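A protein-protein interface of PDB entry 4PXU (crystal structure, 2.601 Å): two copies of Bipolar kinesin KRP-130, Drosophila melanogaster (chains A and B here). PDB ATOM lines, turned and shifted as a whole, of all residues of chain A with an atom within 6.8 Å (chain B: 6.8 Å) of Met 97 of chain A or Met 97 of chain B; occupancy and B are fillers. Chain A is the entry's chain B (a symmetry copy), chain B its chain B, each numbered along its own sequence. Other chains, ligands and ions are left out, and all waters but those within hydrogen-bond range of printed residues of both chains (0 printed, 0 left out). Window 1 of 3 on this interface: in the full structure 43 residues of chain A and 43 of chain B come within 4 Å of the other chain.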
ATOM      1  N   ALA A  92     -11.439  21.272 -17.590  1.00  0.00           N
ATOM      2  CA  ALA A  92     -11.840  21.374 -18.986  1.00  0.00           C
ATOM      3  C   ALA A  92     -11.235  22.615 -19.636  1.00  0.00           C
ATOM      4  O   ALA A  92     -10.798  22.585 -20.787  1.00  0.00           O
ATOM      5  CB  ALA A  92     -13.347  21.404 -19.102  1.00  0.00           C
ATOM      6  N   LEU A  93     -11.214  23.703 -18.877  1.00  0.00           N
ATOM      7  CA  LEU A  93     -10.676  24.975 -19.345  1.00  0.00           C
ATOM      8  C   LEU A  93      -9.185  24.896 -19.662  1.00  0.00           C
ATOM      9  O   LEU A  93      -8.751  25.309 -20.732  1.00  0.00           O
ATOM     10  CB  LEU A  93     -10.916  26.048 -18.290  1.00  0.00           C
ATOM     11  CG  LEU A  93     -10.205  27.383 -18.460  1.00  0.00           C
ATOM     12  CD1 LEU A  93     -10.694  28.073 -19.728  1.00  0.00           C
ATOM     13  CD2 LEU A  93     -10.438  28.247 -17.221  1.00  0.00           C
ATOM     14  N   LEU A  94      -8.409  24.354 -18.726  1.00  0.00           N
ATOM     15  CA  LEU A  94      -6.969  24.226 -18.908  1.00  0.00           C
ATOM     16  C   LEU A  94      -6.622  23.276 -20.040  1.00  0.00           C
ATOM     17  O   LEU A  94      -5.672  23.508 -20.779  1.00  0.00           O
ATOM     18  CB  LEU A  94      -6.301  23.755 -17.613  1.00  0.00           C
ATOM     19  CG  LEU A  94      -6.310  24.832 -16.533  1.00  0.00           C
ATOM     20  CD1 LEU A  94      -6.016  24.229 -15.181  1.00  0.00           C
ATOM     21  CD2 LEU A  94      -5.322  25.944 -16.877  1.00  0.00           C
ATOM     22  N   GLU A  95      -7.391  22.207 -20.173  1.00  0.00           N
ATOM     23  CA  GLU A  95      -7.171  21.260 -21.252  1.00  0.00           C
ATOM     24  C   GLU A  95      -7.377  21.945 -22.602  1.00  0.00           C
ATOM     25  O   GLU A  95      -6.536  21.857 -23.487  1.00  0.00           O
ATOM     26  CB  GLU A  95      -8.100  20.062 -21.099  1.00  0.00           C
ATOM     27  CG  GLU A  95      -7.775  18.923 -22.035  1.00  0.00           C
ATOM     28  CD  GLU A  95      -8.728  17.761 -21.871  1.00  0.00           C
ATOM     29  OE1 GLU A  95      -9.168  17.502 -20.722  1.00  0.00           O
ATOM     30  OE2 GLU A  95      -9.046  17.120 -22.897  1.00  0.00           O
ATOM     31  N   SER A  96      -8.499  22.642 -22.732  1.00  0.00           N
ATOM     32  CA  SER A  96      -8.808  23.409 -23.916  1.00  0.00           C
ATOM     33  C   SER A  96      -7.725  24.460 -24.211  1.00  0.00           C
ATOM     34  O   SER A  96      -7.337  24.659 -25.354  1.00  0.00           O
ATOM     35  CB  SER A  96     -10.163  24.084 -23.753  1.00  0.00           C
ATOM     36  OG  SER A  96     -10.353  25.072 -24.745  1.00  0.00           O
ATOM     37  N   MET A  97      -7.247  25.127 -23.173  1.00  0.00           N
ATOM     38  CA  MET A  97      -6.216  26.144 -23.318  1.00  0.00           C
ATOM     39  C   MET A  97      -4.937  25.499 -23.800  1.00  0.00           C
ATOM     40  O   MET A  97      -4.275  26.002 -24.696  1.00  0.00           O
ATOM     41  CB  MET A  97      -5.979  26.877 -22.001  1.00  0.00           C
ATOM     42  CG  MET A  97      -5.113  28.110 -22.176  1.00  0.00           C
ATOM     43  SD  MET A  97      -3.365  27.904 -21.831  1.00  0.00           S
ATOM     44  CE  MET A  97      -3.377  27.317 -20.166  1.00  0.00           C
ATOM     45  N   MET A  98      -4.588  24.375 -23.190  1.00  0.00           N
ATOM     46  CA  MET A  98      -3.396  23.647 -23.600  1.00  0.00           C
ATOM     47  C   MET A  98      -3.457  23.139 -25.029  1.00  0.00           C
ATOM     48  O   MET A  98      -2.446  23.149 -25.728  1.00  0.00           O
ATOM     49  CB  MET A  98      -3.151  22.474 -22.663  1.00  0.00           C
ATOM     50  CG  MET A  98      -2.503  22.884 -21.355  1.00  0.00           C
ATOM     51  SD  MET A  98      -0.816  23.459 -21.623  1.00  0.00           S
ATOM     52  CE  MET A  98      -1.102  25.214 -21.536  1.00  0.00           C
ATOM     53  N   MET A  99      -4.645  22.711 -25.451  1.00  0.00           N
ATOM     54  CA  MET A  99      -4.876  22.244 -26.807  1.00  0.00           C
ATOM     55  C   MET A  99      -4.567  23.350 -27.792  1.00  0.00           C
ATOM     56  O   MET A  99      -3.771  23.177 -28.699  1.00  0.00           O
ATOM     57  CB  MET A  99      -6.323  21.776 -26.985  1.00  0.00           C
ATOM     58  CG  MET A  99      -6.556  20.812 -28.156  1.00  0.00           C
ATOM     59  SD  MET A  99      -6.147  19.095 -27.802  1.00  0.00           S
ATOM     60  CE  MET A  99      -7.391  18.725 -26.565  1.00  0.00           C
ATOM     61  N   GLN A 100      -5.214  24.490 -27.611  1.00  0.00           N
ATOM     62  CA  GLN A 100      -5.041  25.618 -28.508  1.00  0.00           C
ATOM     63  C   GLN A 100      -3.610  26.117 -28.467  1.00  0.00           C
ATOM     64  O   GLN A 100      -3.038  26.513 -29.480  1.00  0.00           O
ATOM     65  CB  GLN A 100      -6.017  26.710 -28.129  1.00  0.00           C
ATOM     66  CG  GLN A 100      -7.441  26.189 -28.146  1.00  0.00           C
ATOM     67  CD  GLN A 100      -8.483  27.273 -28.093  1.00  0.00           C
ATOM     68  OE1 GLN A 100      -8.600  28.084 -29.012  1.00  0.00           O
ATOM     69  NE2 GLN A 100      -9.239  27.310 -26.998  1.00  0.00           N
ATOM     70  N   MET A 101      -3.036  26.068 -27.281  1.00  0.00           N
ATOM     71  CA  MET A 101      -1.661  26.457 -27.072  1.00  0.00           C
ATOM     72  C   MET A 101      -0.712  25.548 -27.859  1.00  0.00           C
ATOM     73  O   MET A 101       0.328  25.983 -28.355  1.00  0.00           O
ATOM     74  CB  MET A 101      -1.349  26.393 -25.583  1.00  0.00           C
ATOM     75  CG  MET A 101      -0.399  27.437 -25.112  1.00  0.00           C
ATOM     76  SD  MET A 101      -1.053  29.088 -25.334  1.00  0.00           S
ATOM     77  CE  MET A 101       0.396  29.959 -24.752  1.00  0.00           C
ATOM     78  N   GLU A 102      -1.078  24.282 -27.982  1.00  0.00           N
ATOM     79  CA  GLU A 102      -0.246  23.339 -28.704  1.00  0.00           C
ATOM     80  C   GLU A 102      -0.340  23.553 -30.220  1.00  0.00           C
ATOM     81  O   GLU A 102       0.658  23.418 -30.923  1.00  0.00           O
ATOM     82  CB  GLU A 102      -0.619  21.904 -28.340  1.00  0.00           C
ATOM     83  CG  GLU A 102       0.326  20.860 -28.927  1.00  0.00           C
ATOM     84  CD  GLU A 102       1.670  20.810 -28.220  1.00  0.00           C
ATOM     85  OE1 GLU A 102       1.803  21.411 -27.127  1.00  0.00           O
ATOM     86  OE2 GLU A 102       2.599  20.180 -28.773  1.00  0.00           O
ATOM     87  N   ALA B  92      -4.712  36.741 -26.965  1.00  0.00           N
ATOM     88  CA  ALA B  92      -6.153  36.721 -26.754  1.00  0.00           C
ATOM     89  C   ALA B  92      -6.573  35.472 -25.985  1.00  0.00           C
ATOM     90  O   ALA B  92      -7.437  35.521 -25.109  1.00  0.00           O
ATOM     91  CB  ALA B  92      -6.881  36.791 -28.077  1.00  0.00           C
ATOM     92  N   LEU B  93      -5.943  34.355 -26.324  1.00  0.00           N
ATOM     93  CA  LEU B  93      -6.226  33.071 -25.693  1.00  0.00           C
ATOM     94  C   LEU B  93      -5.896  33.069 -24.204  1.00  0.00           C
ATOM     95  O   LEU B  93      -6.716  32.673 -23.382  1.00  0.00           O
ATOM     96  CB  LEU B  93      -5.434  31.974 -26.392  1.00  0.00           C
ATOM     97  CG  LEU B  93      -5.380  30.604 -25.730  1.00  0.00           C
ATOM     98  CD1 LEU B  93      -6.778  29.998 -25.677  1.00  0.00           C
ATOM     99  CD2 LEU B  93      -4.404  29.707 -26.491  1.00  0.00           C
ATOM    100  N   LEU B  94      -4.691  33.522 -23.864  1.00  0.00           N
ATOM    101  CA  LEU B  94      -4.255  33.566 -22.475  1.00  0.00           C
ATOM    102  C   LEU B  94      -5.081  34.538 -21.651  1.00  0.00           C
ATOM    103  O   LEU B  94      -5.376  34.276 -20.490  1.00  0.00           O
ATOM    104  CB  LEU B  94      -2.773  33.941 -22.385  1.00  0.00           C
ATOM    105  CG  LEU B  94      -1.863  32.824 -22.884  1.00  0.00           C
ATOM    106  CD1 LEU B  94      -0.475  33.351 -23.154  1.00  0.00           C
ATOM    107  CD2 LEU B  94      -1.839  31.666 -21.889  1.00  0.00           C
ATOM    108  N   GLU B  95      -5.451  35.658 -22.252  1.00  0.00           N
ATOM    109  CA  GLU B  95      -6.282  36.632 -21.565  1.00  0.00           C
ATOM    110  C   GLU B  95      -7.637  36.017 -21.220  1.00  0.00           C
ATOM    111  O   GLU B  95      -8.090  36.087 -20.085  1.00  0.00           O
ATOM    112  CB  GLU B  95      -6.449  37.880 -22.425  1.00  0.00           C
ATOM    113  CG  GLU B  95      -7.094  39.032 -21.694  1.00  0.00           C
ATOM    114  CD  GLU B  95      -7.265  40.245 -22.582  1.00  0.00           C
ATOM    115  OE1 GLU B  95      -6.385  40.484 -23.447  1.00  0.00           O
ATOM    116  OE2 GLU B  95      -8.288  40.945 -22.419  1.00  0.00           O
ATOM    117  N   SER B  96      -8.261  35.398 -22.214  1.00  0.00           N
ATOM    118  CA  SER B  96      -9.514  34.700 -22.036  1.00  0.00           C
ATOM    119  C   SER B  96      -9.402  33.596 -20.972  1.00  0.00           C
ATOM    120  O   SER B  96     -10.293  33.420 -20.153  1.00  0.00           O
ATOM    121  CB  SER B  96      -9.966  34.106 -23.363  1.00  0.00           C
ATOM    122  OG  SER B  96     -11.009  33.174 -23.164  1.00  0.00           O
ATOM    123  N   MET B  97      -8.303  32.859 -20.995  1.00  0.00           N
ATOM    124  CA  MET B  97      -8.075  31.785 -20.039  1.00  0.00           C
ATOM    125  C   MET B  97      -7.946  32.367 -18.650  1.00  0.00           C
ATOM    126  O   MET B  97      -8.519  31.860 -17.697  1.00  0.00           O
ATOM    127  CB  MET B  97      -6.826  30.986 -20.400  1.00  0.00           C
ATOM    128  CG  MET B  97      -6.706  29.709 -19.590  1.00  0.00           C
ATOM    129  SD  MET B  97      -5.660  29.790 -18.135  1.00  0.00           S
ATOM    130  CE  MET B  97      -4.114  30.308 -18.813  1.00  0.00           C
ATOM    131  N   MET B  98      -7.176  33.441 -18.540  1.00  0.00           N
ATOM    132  CA  MET B  98      -7.012  34.109 -17.256  1.00  0.00           C
ATOM    133  C   MET B  98      -8.305  34.678 -16.699  1.00  0.00           C
ATOM    134  O   MET B  98      -8.524  34.632 -15.491  1.00  0.00           O
ATOM    135  CB  MET B  98      -5.985  35.225 -17.375  1.00  0.00           C
ATOM    136  CG  MET B  98      -4.555  34.722 -17.345  1.00  0.00           C
ATOM    137  SD  MET B  98      -4.140  34.053 -15.724  1.00  0.00           S
ATOM    138  CE  MET B  98      -4.290  32.317 -16.091  1.00  0.00           C
ATOM    139  N   MET B  99      -9.150  35.196 -17.586  1.00  0.00           N
ATOM    140  CA  MET B  99     -10.448  35.732 -17.215  1.00  0.00           C
ATOM    141  C   MET B  99     -11.286  34.650 -16.570  1.00  0.00           C
ATOM    142  O   MET B  99     -11.772  34.809 -15.464  1.00  0.00           O
ATOM    143  CB  MET B  99     -11.176  36.297 -18.438  1.00  0.00           C
ATOM    144  CG  MET B  99     -12.276  37.321 -18.124  1.00  0.00           C
ATOM    145  SD  MET B  99     -11.678  38.992 -17.830  1.00  0.00           S
ATOM    146  CE  MET B  99     -11.042  39.390 -19.459  1.00  0.00           C
ATOM    147  N   GLN B 100     -11.460  33.546 -17.280  1.00  0.00           N
ATOM    148  CA  GLN B 100     -12.275  32.447 -16.797  1.00  0.00           C
ATOM    149  C   GLN B 100     -11.680  31.858 -15.534  1.00  0.00           C
ATOM    150  O   GLN B 100     -12.390  31.467 -14.610  1.00  0.00           O
ATOM    151  CB  GLN B 100     -12.401  31.404 -17.885  1.00  0.00           C
ATOM    152  CG  GLN B 100     -12.971  32.015 -19.152  1.00  0.00           C
ATOM    153  CD  GLN B 100     -13.421  30.997 -20.164  1.00  0.00           C
ATOM    154  OE1 GLN B 100     -14.355  30.233 -19.923  1.00  0.00           O
ATOM    155  NE2 GLN B 100     -12.739  30.964 -21.308  1.00  0.00           N
ATOM    156  N   MET B 101     -10.363  31.821 -15.501  1.00  0.00           N
ATOM    157  CA  MET B 101      -9.631  31.338 -14.353  1.00  0.00           C
ATOM    158  C   MET B 101      -9.898  32.217 -13.128  1.00  0.00           C
ATOM    159  O   MET B 101      -9.947  31.738 -11.995  1.00  0.00           O
ATOM    160  CB  MET B 101      -8.145  31.322 -14.685  1.00  0.00           C
ATOM    161  CG  MET B 101      -7.391  30.202 -14.059  1.00  0.00           C
ATOM    162  SD  MET B 101      -7.967  28.606 -14.629  1.00  0.00           S
ATOM    163  CE  MET B 101      -6.895  27.622 -13.588  1.00  0.00           C
ATOM    164  N   GLU B 102     -10.080  33.508 -13.359  1.00  0.00           N
ATOM    165  CA  GLU B 102     -10.335  34.424 -12.264  1.00  0.00           C
ATOM    166  C   GLU B 102     -11.765  34.278 -11.730  1.00  0.00           C
ATOM    167  O   GLU B 102     -11.985  34.379 -10.525  1.00  0.00           O
ATOM    168  CB  GLU B 102     -10.066  35.865 -12.695  1.00  0.00           C
ATOM    169  CG  GLU B 102     -10.145  36.869 -11.551  1.00  0.00           C
ATOM    170  CD  GLU B 102      -8.946  36.806 -10.620  1.00  0.00           C
ATOM    171  OE1 GLU B 102      -7.935  36.154 -10.977  1.00  0.00           O
ATOM    172  OE2 GLU B 102      -9.026  37.397  -9.520  1.00  0.00           O
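Hydrophobic or aromatic side chains of chain A within 4 Å of the printed part of chain B: Leu 93, Leu 94, Met 97 and Met 101.
Hydrophobic or aromatic side chains of chain B that line the printed part of chain A: Leu 93, Leu 94, Met 97 and Met 101.
Among the printed residues, 7 pairs touch across the chains.
Among the printed residues, pairs that only touch across the chains: Met 97 of chain A with Met 97 of chain B (3.4 Å), Met 101 of chain A with Leu 93 of chain B (3.6 Å), Leu 93 of chain A with Met 101 of chain B (3.6 Å), Leu 93 of chain A with Gln 100 of chain B (3.8 Å), Gln 100 of chain A with Leu 93 of chain B (3.8 Å), Met 101 of chain A with Leu 94 of chain B (3.8 Å) and Leu 94 of chain A with Met 101 of chain B (3.9 Å).
The side-chain hydroxyl (OG) of Ser 96 of chain B lies within hydrogen-bond range of the side-chain amide nitrogen (NE2) of Gln 100 of chain B (3.4 Å).
The side-chain hydroxyl of Ser 96 of chain A sits at hydrogen-bond distance from the side-chain amide nitrogen of Gln 100 of chain A, 3.4 Å away.
Leu 93 of chain A touches Gln 100 of chain B, and with the chains exchanged Gln 100 of chain A touches Leu 93 of chain B.
Leu 93 of chain A touches Met 101 of chain B, and with the chains exchanged Met 101 of chain A touches Leu 93 of chain B.
Leu 94 of chain A touches Met 101 of chain B, and with the chains exchanged Met 101 of chain A touches Leu 94 of chain B.
Met 97 of chain A touches its own counterpart, Met 97 of chain B.
11 positions are printed for both chains.
Of the 7 pairs that touch across the chains among the printed residues, 7 have their exchanged pair printed and touching as well.
Met 97 of chain A touches one residue of chain B.
Of the printed residues of chain B, Gln 100 of chain A touches Leu 93.
Of the printed residues of chain B, Met 101 of chain A touches Leu 93 (3.6 Å) and Leu 94 (3.8 Å).
Of the printed residues of chain A, Leu 93 of chain B touches Gln 100 (3.8 Å) and Met 101 (3.6 Å).
Printed residues of chain A within 4 Å of Leu 94 of chain B: Met 101.
Of the printed residues of chain A, Met 97 of chain B touches Met 97 (3.4 Å).
The nearest residue of chain B that does not touch Met 97 of chain A is Leu 94 of chain B (4.1 Å).
The nearest printed residue of chain A that does not touch Gln 100 of chain B is Ser 96 of chain A (7.2 Å).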
